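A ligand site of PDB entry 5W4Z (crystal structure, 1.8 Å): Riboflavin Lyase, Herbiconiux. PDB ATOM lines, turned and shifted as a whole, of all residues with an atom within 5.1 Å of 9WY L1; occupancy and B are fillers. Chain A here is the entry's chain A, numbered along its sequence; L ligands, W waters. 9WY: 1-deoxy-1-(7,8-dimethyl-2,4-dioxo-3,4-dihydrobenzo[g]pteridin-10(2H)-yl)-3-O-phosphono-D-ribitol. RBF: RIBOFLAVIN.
Residues that only touch 9WY L1: Ala 63 (3.4 Å), Val 141 (3.5 Å), Ala 232 (3.4 Å), Gly 233 (3.4 Å), Ser 234 (3.5 Å), Phe 250 (3.4 Å), Leu 341 (3.8 Å) and Gln 343 (3.6 Å).
Hydrophobic or aromatic side chains that line 9WY L1: Ala 63, Val 141, His 160, Tyr 164, Ala 232 and Phe 250.
The nearest printed residue that does not touch 9WY L1 is Gly 252 (4.1 Å).
Water W4 lies within hydrogen-bond range of an oxygen (O2P) of 9WY L1 (2.5 Å), the backbone NH of Ser 234 (2.9 Å) and the side-chain hydroxyl of Thr 344 (3.0 Å).
Water W1 lies within hydrogen-bond range of an oxygen (O2') of 9WY L1 (2.9 Å), an oxygen (O4) of RBF L2 (3.0 Å), the backbone NH of Thr 344 (3.0 Å) and the backbone NH of Gln 343 (3.5 Å).
Water W2 lies within hydrogen-bond range of the side-chain hydroxyl of Thr 143 (3.0 Å) and an oxygen (O2) of 9WY L1 (3.4 Å).
Water W3 bridges the backbone NH (N) of Gly 144 (3.4 Å) and an oxygen (O2) of 9WY L1 (3.4 Å).
An oxygen (O1P) of 9WY L1 is in hydrogen-bond range of a ring nitrogen (NE2) of His 160 (2.6 Å).
N of Ser 235 lies within hydrogen-bond range of O3P of 9WY L1 (3.1 Å).
The side-chain hydroxyl of Ser 235 lies within hydrogen-bond range of an oxygen (O3P) of 9WY L1 (2.7 Å).
The guanidinium group (NH2) of Arg 163 lies within hydrogen-bond range of an oxygen (O5') of 9WY L1, 2.7 Å away.
The backbone carbonyl oxygen of Thr 142 lies within hydrogen-bond range of an oxygen (O5') of 9WY L1 (3.5 Å).
OG1 of Thr 142 sits at hydrogen-bond distance from O5' of 9WY L1.
The backbone NH (N) of Gly 144 lies within hydrogen-bond range of an oxygen (O4') of 9WY L1 (2.8 Å).
An oxygen (O2P) of 9WY L1 is in hydrogen-bond range of the side-chain hydroxyl of Thr 344 (2.9 Å).
The side-chain hydroxyl (OH) of Tyr 164 lies within hydrogen-bond range of an oxygen (O3P) of 9WY L1 (2.9 Å).
N of Asp 64 lies within hydrogen-bond range of O4 of 9WY L1, at 3.3 Å.
N3 of 9WY L1 is in hydrogen-bond range of O of Asp 64 (3.0 Å).
An oxygen (O5') of 9WY L1 is in hydrogen-bond range of the backbone carbonyl oxygen (O) of Thr 143 (3.1 Å).
The backbone NH (N) of Asp 64 is in hydrogen-bond range of an oxygen (O5') of RBF L2 (3.5 Å).
O4' of RBF L2 sits at hydrogen-bond distance from O of Asp 64, 3.0 Å away.
The side-chain hydroxyl (OG) of Ser 342 lies within hydrogen-bond range of a nitrogen (N3) of RBF L2, at 3.1 Å.
O4 of RBF L2 lies within hydrogen-bond range of O2' of 9WY L1 (2.7 Å).
ND1 of His 160 lies close to OE1 of Gln 343, 3.3 Å away.
OG of Ser 235 sits at hydrogen-bond distance from N of Gly 238 (3.1 Å).
The backbone carbonyl oxygen (O) of Thr 142 sits at hydrogen-bond distance from the guanidinium group (NE) of Arg 163 (2.8 Å).
The guanidinium group (NH2) of Arg 163 lies within hydrogen-bond range of the backbone carbonyl oxygen (O) of Leu 341.
The backbone carbonyl oxygen (O) of Gly 144 lies within hydrogen-bond range of the side-chain hydroxyl (OG) of Ser 342.
OG of Ser 234 sits at hydrogen-bond distance from OG1 of Thr 344.
OD1 of Asn 139 lies within hydrogen-bond range of N of Ala 232 (3.5 Å).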
ATOM      1  N   ALA A  63      10.641  24.105  14.331  1.00  0.00           N
ATOM      2  CA  ALA A  63       9.625  23.109  14.653  1.00  0.00           C
ATOM      3  C   ALA A  63      10.253  22.017  15.512  1.00  0.00           C
ATOM      4  O   ALA A  63      11.456  22.021  15.776  1.00  0.00           O
ATOM      5  CB  ALA A  63       9.021  22.524  13.373  1.00  0.00           C
ATOM      6  N   ASP A  64       9.445  21.054  15.961  1.00  0.00           N
ATOM      7  CA  ASP A  64      10.009  19.918  16.672  1.00  0.00           C
ATOM      8  C   ASP A  64       9.125  18.694  16.457  1.00  0.00           C
ATOM      9  O   ASP A  64       7.957  18.805  16.076  1.00  0.00           O
ATOM     10  CB  ASP A  64      10.161  20.226  18.168  1.00  0.00           C
ATOM     11  CG  ASP A  64      11.048  19.213  18.922  1.00  0.00           C
ATOM     12  OD1 ASP A  64      11.918  18.561  18.283  1.00  0.00           O
ATOM     13  OD2 ASP A  64      10.870  19.086  20.153  1.00  0.00           O
ATOM     14  N   THR A 110       9.792  25.232  19.187  1.00  0.00           N
ATOM     15  CA  THR A 110       8.646  24.395  19.524  1.00  0.00           C
ATOM     16  C   THR A 110       8.936  23.576  20.781  1.00  0.00           C
ATOM     17  O   THR A 110      10.053  23.089  20.979  1.00  0.00           O
ATOM     18  CB  THR A 110       8.307  23.488  18.339  1.00  0.00           C
ATOM     19  OG1 THR A 110       7.783  24.298  17.273  1.00  0.00           O
ATOM     20  CG2 THR A 110       7.270  22.456  18.720  1.00  0.00           C
ATOM     21  N   ASN A 139       6.822  27.954  20.724  1.00  0.00           N
ATOM     22  CA  ASN A 139       5.683  27.453  19.962  1.00  0.00           C
ATOM     23  C   ASN A 139       5.051  26.277  20.715  1.00  0.00           C
ATOM     24  O   ASN A 139       5.640  25.191  20.808  1.00  0.00           O
ATOM     25  CB  ASN A 139       6.084  27.043  18.553  1.00  0.00           C
ATOM     26  CG  ASN A 139       4.911  26.527  17.746  1.00  0.00           C
ATOM     27  OD1 ASN A 139       3.828  27.116  17.761  1.00  0.00           O
ATOM     28  ND2 ASN A 139       5.107  25.401  17.087  1.00  0.00           N
ATOM     29  N   VAL A 141       2.921  23.225  21.285  1.00  0.00           N
ATOM     30  CA  VAL A 141       2.258  22.139  20.563  1.00  0.00           C
ATOM     31  C   VAL A 141       1.885  21.043  21.541  1.00  0.00           C
ATOM     32  O   VAL A 141       2.434  20.931  22.635  1.00  0.00           O
ATOM     33  CB  VAL A 141       3.122  21.571  19.420  1.00  0.00           C
ATOM     34  CG1 VAL A 141       3.454  22.651  18.385  1.00  0.00           C
ATOM     35  CG2 VAL A 141       4.394  20.918  19.963  1.00  0.00           C
ATOM     36  N   THR A 142       0.924  20.220  21.136  1.00  0.00           N
ATOM     37  CA  THR A 142       0.530  19.042  21.901  1.00  0.00           C
ATOM     38  C   THR A 142       1.077  17.747  21.295  1.00  0.00           C
ATOM     39  O   THR A 142       0.608  16.667  21.666  1.00  0.00           O
ATOM     40  CB  THR A 142      -0.989  18.974  22.019  1.00  0.00           C
ATOM     41  OG1 THR A 142      -1.575  19.113  20.722  1.00  0.00           O
ATOM     42  CG2 THR A 142      -1.508  20.101  22.911  1.00  0.00           C
ATOM     43  N   THR A 143       2.030  17.852  20.347  1.00  0.00           N
ATOM     44  CA  THR A 143       2.777  16.742  19.745  1.00  0.00           C
ATOM     45  C   THR A 143       1.946  15.923  18.768  1.00  0.00           C
ATOM     46  O   THR A 143       1.049  15.161  19.169  1.00  0.00           O
ATOM     47  CB  THR A 143       3.395  15.855  20.817  1.00  0.00           C
ATOM     48  OG1 THR A 143       4.333  16.632  21.558  1.00  0.00           O
ATOM     49  CG2 THR A 143       4.135  14.638  20.202  1.00  0.00           C
ATOM     50  N   GLY A 144       2.239  16.058  17.474  1.00  0.00           N
ATOM     51  CA  GLY A 144       1.529  15.331  16.426  1.00  0.00           C
ATOM     52  C   GLY A 144       2.002  13.919  16.208  1.00  0.00           C
ATOM     53  O   GLY A 144       1.387  13.174  15.437  1.00  0.00           O
ATOM     54  N   HIS A 160      -6.556  13.120  21.745  1.00  0.00           N
ATOM     55  CA  HIS A 160      -6.272  14.409  21.097  1.00  0.00           C
ATOM     56  C   HIS A 160      -6.794  15.587  21.925  1.00  0.00           C
ATOM     57  O   HIS A 160      -6.028  16.471  22.302  1.00  0.00           O
ATOM     58  CB  HIS A 160      -6.866  14.432  19.693  1.00  0.00           C
ATOM     59  CG  HIS A 160      -6.681  15.742  18.974  1.00  0.00           C
ATOM     60  ND1 HIS A 160      -7.553  16.798  19.112  1.00  0.00           N
ATOM     61  CD2 HIS A 160      -5.718  16.153  18.113  1.00  0.00           C
ATOM     62  CE1 HIS A 160      -7.147  17.806  18.367  1.00  0.00           C
ATOM     63  NE2 HIS A 160      -6.036  17.445  17.746  1.00  0.00           N
ATOM     64  N   ARG A 163      -5.193  16.208  25.190  1.00  0.00           N
ATOM     65  CA  ARG A 163      -3.872  16.826  25.182  1.00  0.00           C
ATOM     66  C   ARG A 163      -3.983  18.343  25.269  1.00  0.00           C
ATOM     67  O   ARG A 163      -3.099  19.000  25.830  1.00  0.00           O
ATOM     68  CB  ARG A 163      -3.070  16.403  23.943  1.00  0.00           C
ATOM     69  CG  ARG A 163      -2.691  14.914  23.900  1.00  0.00           C
ATOM     70  CD  ARG A 163      -1.486  14.606  22.995  1.00  0.00           C
ATOM     71  NE  ARG A 163      -1.683  15.022  21.606  1.00  0.00           N
ATOM     72  CZ  ARG A 163      -2.356  14.313  20.704  1.00  0.00           C
ATOM     73  NH1 ARG A 163      -2.906  13.150  21.040  1.00  0.00           N
ATOM     74  NH2 ARG A 163      -2.481  14.772  19.459  1.00  0.00           N
ATOM     75  N   TYR A 164      -5.055  18.917  24.721  1.00  0.00           N
ATOM     76  CA  TYR A 164      -5.259  20.353  24.865  1.00  0.00           C
ATOM     77  C   TYR A 164      -5.744  20.726  26.269  1.00  0.00           C
ATOM     78  O   TYR A 164      -5.370  21.785  26.784  1.00  0.00           O
ATOM     79  CB  TYR A 164      -6.222  20.852  23.791  1.00  0.00           C
ATOM     80  CG  TYR A 164      -5.548  21.033  22.445  1.00  0.00           C
ATOM     81  CD1 TYR A 164      -4.657  22.091  22.243  1.00  0.00           C
ATOM     82  CD2 TYR A 164      -5.773  20.151  21.401  1.00  0.00           C
ATOM     83  CE1 TYR A 164      -4.017  22.264  21.016  1.00  0.00           C
ATOM     84  CE2 TYR A 164      -5.138  20.323  20.162  1.00  0.00           C
ATOM     85  CZ  TYR A 164      -4.269  21.385  19.985  1.00  0.00           C
ATOM     86  OH  TYR A 164      -3.625  21.565  18.764  1.00  0.00           O
ATOM     87  N   ALA A 232       0.462  26.450  17.383  1.00  0.00           N
ATOM     88  CA  ALA A 232       0.284  25.765  16.110  1.00  0.00           C
ATOM     89  C   ALA A 232      -0.573  24.538  16.353  1.00  0.00           C
ATOM     90  O   ALA A 232      -0.188  23.647  17.121  1.00  0.00           O
ATOM     91  CB  ALA A 232       1.639  25.394  15.490  1.00  0.00           C
ATOM     92  N   GLY A 233      -1.705  24.463  15.667  1.00  0.00           N
ATOM     93  CA  GLY A 233      -2.667  23.413  15.903  1.00  0.00           C
ATOM     94  C   GLY A 233      -4.044  23.957  15.566  1.00  0.00           C
ATOM     95  O   GLY A 233      -4.658  24.642  16.387  1.00  0.00           O
ATOM     96  N   SER A 234      -4.535  23.684  14.356  1.00  0.00           N
ATOM     97  CA  SER A 234      -5.725  24.341  13.845  1.00  0.00           C
ATOM     98  C   SER A 234      -6.950  23.423  13.847  1.00  0.00           C
ATOM     99  O   SER A 234      -7.911  23.681  13.115  1.00  0.00           O
ATOM    100  CB  SER A 234      -5.481  24.895  12.442  1.00  0.00           C
ATOM    101  OG  SER A 234      -5.224  23.855  11.514  1.00  0.00           O
ATOM    102  N   SER A 235      -6.942  22.370  14.655  1.00  0.00           N
ATOM    103  CA  SER A 235      -8.186  21.663  14.921  1.00  0.00           C
ATOM    104  C   SER A 235      -9.105  22.600  15.693  1.00  0.00           C
ATOM    105  O   SER A 235      -8.686  23.624  16.244  1.00  0.00           O
ATOM    106  CB  SER A 235      -7.951  20.387  15.720  1.00  0.00           C
ATOM    107  OG  SER A 235      -7.396  20.675  16.992  1.00  0.00           O
ATOM    108  N   GLY A 238      -7.889  23.044  18.987  1.00  0.00           N
ATOM    109  CA  GLY A 238      -6.647  23.804  18.987  1.00  0.00           C
ATOM    110  C   GLY A 238      -6.860  25.294  18.770  1.00  0.00           C
ATOM    111  O   GLY A 238      -6.123  26.116  19.313  1.00  0.00           O
ATOM    112  N   PHE A 250       0.266  30.211  14.238  1.00  0.00           N
ATOM    113  CA  PHE A 250       0.852  29.690  13.013  1.00  0.00           C
ATOM    114  C   PHE A 250      -0.213  28.861  12.297  1.00  0.00           C
ATOM    115  O   PHE A 250      -0.673  27.853  12.833  1.00  0.00           O
ATOM    116  CB  PHE A 250       2.084  28.855  13.396  1.00  0.00           C
ATOM    117  CG  PHE A 250       2.970  28.469  12.233  1.00  0.00           C
ATOM    118  CD1 PHE A 250       2.832  29.050  10.979  1.00  0.00           C
ATOM    119  CD2 PHE A 250       3.969  27.497  12.413  1.00  0.00           C
ATOM    120  CE1 PHE A 250       3.664  28.677   9.935  1.00  0.00           C
ATOM    121  CE2 PHE A 250       4.797  27.117  11.363  1.00  0.00           C
ATOM    122  CZ  PHE A 250       4.642  27.714  10.117  1.00  0.00           C
ATOM    123  N   LEU A 251      -0.614  29.303  11.107  1.00  0.00           N
ATOM    124  CA  LEU A 251      -1.609  28.610  10.295  1.00  0.00           C
ATOM    125  C   LEU A 251      -0.980  28.012   9.039  1.00  0.00           C
ATOM    126  O   LEU A 251      -0.117  28.643   8.410  1.00  0.00           O
ATOM    127  CB  LEU A 251      -2.733  29.555   9.878  1.00  0.00           C
ATOM    128  CG  LEU A 251      -3.674  30.013  11.001  1.00  0.00           C
ATOM    129  CD1 LEU A 251      -4.700  30.997  10.456  1.00  0.00           C
ATOM    130  CD2 LEU A 251      -4.372  28.808  11.622  1.00  0.00           C
ATOM    131  N   GLY A 252      -1.429  26.821   8.653  1.00  0.00           N
ATOM    132  CA  GLY A 252      -1.036  26.267   7.381  1.00  0.00           C
ATOM    133  C   GLY A 252      -1.631  27.051   6.217  1.00  0.00           C
ATOM    134  O   GLY A 252      -2.557  27.849   6.373  1.00  0.00           O
ATOM    135  N   LEU A 341      -3.974  11.766  16.495  1.00  0.00           N
ATOM    136  CA  LEU A 341      -2.709  12.468  16.346  1.00  0.00           C
ATOM    137  C   LEU A 341      -2.927  13.810  15.660  1.00  0.00           C
ATOM    138  O   LEU A 341      -3.662  14.662  16.184  1.00  0.00           O
ATOM    139  CB  LEU A 341      -1.719  11.596  15.567  1.00  0.00           C
ATOM    140  CG  LEU A 341      -0.881  10.567  16.338  1.00  0.00           C
ATOM    141  CD1 LEU A 341      -1.684   9.843  17.399  1.00  0.00           C
ATOM    142  CD2 LEU A 341      -0.244   9.569  15.382  1.00  0.00           C
ATOM    143  N   SER A 342      -2.323  14.011  14.489  1.00  0.00           N
ATOM    144  CA  SER A 342      -2.440  15.277  13.752  1.00  0.00           C
ATOM    145  C   SER A 342      -3.762  15.266  12.981  1.00  0.00           C
ATOM    146  O   SER A 342      -3.830  14.854  11.828  1.00  0.00           O
ATOM    147  CB  SER A 342      -1.245  15.467  12.825  1.00  0.00           C
ATOM    148  OG  SER A 342      -0.004  15.278  13.521  1.00  0.00           O
ATOM    149  N   GLN A 343      -4.828  15.748  13.644  1.00  0.00           N
ATOM    150  CA  GLN A 343      -6.169  15.634  13.068  1.00  0.00           C
ATOM    151  C   GLN A 343      -6.353  16.505  11.836  1.00  0.00           C
ATOM    152  O   GLN A 343      -7.145  16.168  10.946  1.00  0.00           O
ATOM    153  CB  GLN A 343      -7.224  15.973  14.119  1.00  0.00           C
ATOM    154  CG  GLN A 343      -7.287  14.953  15.242  1.00  0.00           C
ATOM    155  CD  GLN A 343      -8.487  15.160  16.135  1.00  0.00           C
ATOM    156  OE1 GLN A 343      -9.027  16.251  16.214  1.00  0.00           O
ATOM    157  NE2 GLN A 343      -8.916  14.089  16.800  1.00  0.00           N
ATOM    158  N   THR A 344      -5.633  17.635  11.750  1.00  0.00           N
ATOM    159  CA  THR A 344      -5.761  18.492  10.570  1.00  0.00           C
ATOM    160  C   THR A 344      -5.270  17.776   9.308  1.00  0.00           C
ATOM    161  O   THR A 344      -5.834  17.976   8.232  1.00  0.00           O
ATOM    162  CB  THR A 344      -5.015  19.813  10.799  1.00  0.00           C
ATOM    163  OG1 THR A 344      -5.705  20.576  11.793  1.00  0.00           O
ATOM    164  CG2 THR A 344      -4.931  20.624   9.513  1.00  0.00           C
HETATM  165  C10 9WY L   1       2.737  20.871  15.264  1.00  0.00           C
HETATM  166  C7  9WY L   1       1.657  24.362  11.913  1.00  0.00           C
HETATM  167  O3P 9WY L   1      -4.811  20.726  16.239  1.00  0.00           O
HETATM  168  P   9WY L   1      -4.002  19.772  15.520  1.00  0.00           P
HETATM  169  O1P 9WY L   1      -4.494  18.483  15.914  1.00  0.00           O
HETATM  170  O2P 9WY L   1      -4.090  19.984  14.083  1.00  0.00           O
HETATM  171  O5' 9WY L   1      -1.275  17.105  18.799  1.00  0.00           O
HETATM  172  C5' 9WY L   1      -1.822  17.658  17.625  1.00  0.00           C
HETATM  173  C4' 9WY L   1      -0.910  18.696  17.052  1.00  0.00           C
HETATM  174  O4' 9WY L   1       0.387  18.137  16.918  1.00  0.00           O
HETATM  175  C3' 9WY L   1      -1.455  19.068  15.691  1.00  0.00           C
HETATM  176  O3' 9WY L   1      -2.485  20.027  15.895  1.00  0.00           O
HETATM  177  C2' 9WY L   1      -0.352  19.578  14.774  1.00  0.00           C
HETATM  178  O2' 9WY L   1      -0.977  20.029  13.603  1.00  0.00           O
HETATM  179  C1' 9WY L   1       0.314  20.760  15.386  1.00  0.00           C
HETATM  180  N10 9WY L   1       1.521  21.299  14.801  1.00  0.00           N
HETATM  181  C9A 9WY L   1       1.545  22.323  13.854  1.00  0.00           C
HETATM  182  C9  9WY L   1       0.362  22.823  13.348  1.00  0.00           C
HETATM  183  C8  9WY L   1       0.379  23.812  12.398  1.00  0.00           C
HETATM  184  C8M 9WY L   1      -0.900  24.361  11.888  1.00  0.00           C
HETATM  185  C7M 9WY L   1       1.673  25.451  10.887  1.00  0.00           C
HETATM  186  C6  9WY L   1       2.837  23.854  12.413  1.00  0.00           C
HETATM  187  C5A 9WY L   1       2.815  22.858  13.358  1.00  0.00           C
HETATM  188  N5  9WY L   1       3.973  22.385  13.827  1.00  0.00           N
HETATM  189  N1  9WY L   1       2.814  19.908  16.176  1.00  0.00           N
HETATM  190  C4A 9WY L   1       3.973  21.434  14.735  1.00  0.00           C
HETATM  191  C4  9WY L   1       5.216  20.884  15.286  1.00  0.00           C
HETATM  192  O4  9WY L   1       6.289  21.309  14.914  1.00  0.00           O
HETATM  193  N3  9WY L   1       5.149  19.929  16.172  1.00  0.00           N
HETATM  194  C2  9WY L   1       4.010  19.449  16.602  1.00  0.00           C
HETATM  195  O2  9WY L   1       4.041  18.562  17.445  1.00  0.00           O
HETATM  196  N1  RBF L   2       3.867  18.676  12.530  1.00  0.00           N
HETATM  197  C2  RBF L   2       3.012  17.772  13.053  1.00  0.00           C
HETATM  198  O2  RBF L   2       3.397  16.969  13.847  1.00  0.00           O
HETATM  199  N3  RBF L   2       1.703  17.767  12.683  1.00  0.00           N
HETATM  200  C4  RBF L   2       1.261  18.667  11.816  1.00  0.00           C
HETATM  201  O4  RBF L   2       0.133  18.653  11.501  1.00  0.00           O
HETATM  202  C4A RBF L   2       2.122  19.611  11.273  1.00  0.00           C
HETATM  203  N5  RBF L   2       1.656  20.552  10.368  1.00  0.00           N
HETATM  204  C5A RBF L   2       2.496  21.456   9.837  1.00  0.00           C
HETATM  205  C6  RBF L   2       2.022  22.422   8.887  1.00  0.00           C
HETATM  206  C7  RBF L   2       2.904  23.358   8.342  1.00  0.00           C
HETATM  207  C7M RBF L   2       2.322  24.323   7.374  1.00  0.00           C
HETATM  208  C8  RBF L   2       4.248  23.340   8.721  1.00  0.00           C
HETATM  209  C8M RBF L   2       5.282  24.336   8.178  1.00  0.00           C
HETATM  210  C9  RBF L   2       4.717  22.401   9.655  1.00  0.00           C
HETATM  211  C9A RBF L   2       3.822  21.445  10.200  1.00  0.00           C
HETATM  212  N10 RBF L   2       4.283  20.552  11.081  1.00  0.00           N
HETATM  213  C10 RBF L   2       3.425  19.616  11.630  1.00  0.00           C
HETATM  214  C1' RBF L   2       5.658  20.389  11.609  1.00  0.00           C
HETATM  215  C2' RBF L   2       6.547  19.617  10.591  1.00  0.00           C
HETATM  216  O2' RBF L   2       6.038  18.341  10.404  1.00  0.00           O
HETATM  217  C3' RBF L   2       7.988  19.523  11.147  1.00  0.00           C
HETATM  218  O3' RBF L   2       8.891  19.555  10.061  1.00  0.00           O
HETATM  219  C4' RBF L   2       8.151  18.260  11.956  1.00  0.00           C
HETATM  220  O4' RBF L   2       7.426  18.349  13.177  1.00  0.00           O
HETATM  221  C5' RBF L   2       9.651  18.060  12.332  1.00  0.00           C
HETATM  222  O5' RBF L   2      10.094  19.163  13.149  1.00  0.00           O
HETATM  223  O   HOH W   1      -2.699  18.144  12.264  1.00  0.00           O
HETATM  224  O   HOH W   2       6.414  17.446  19.559  1.00  0.00           O
HETATM  225  O   HOH W   3       5.549  15.542  16.931  1.00  0.00           O
HETATM  226  O   HOH W   4      -3.094  21.823  12.742  1.00  0.00           O
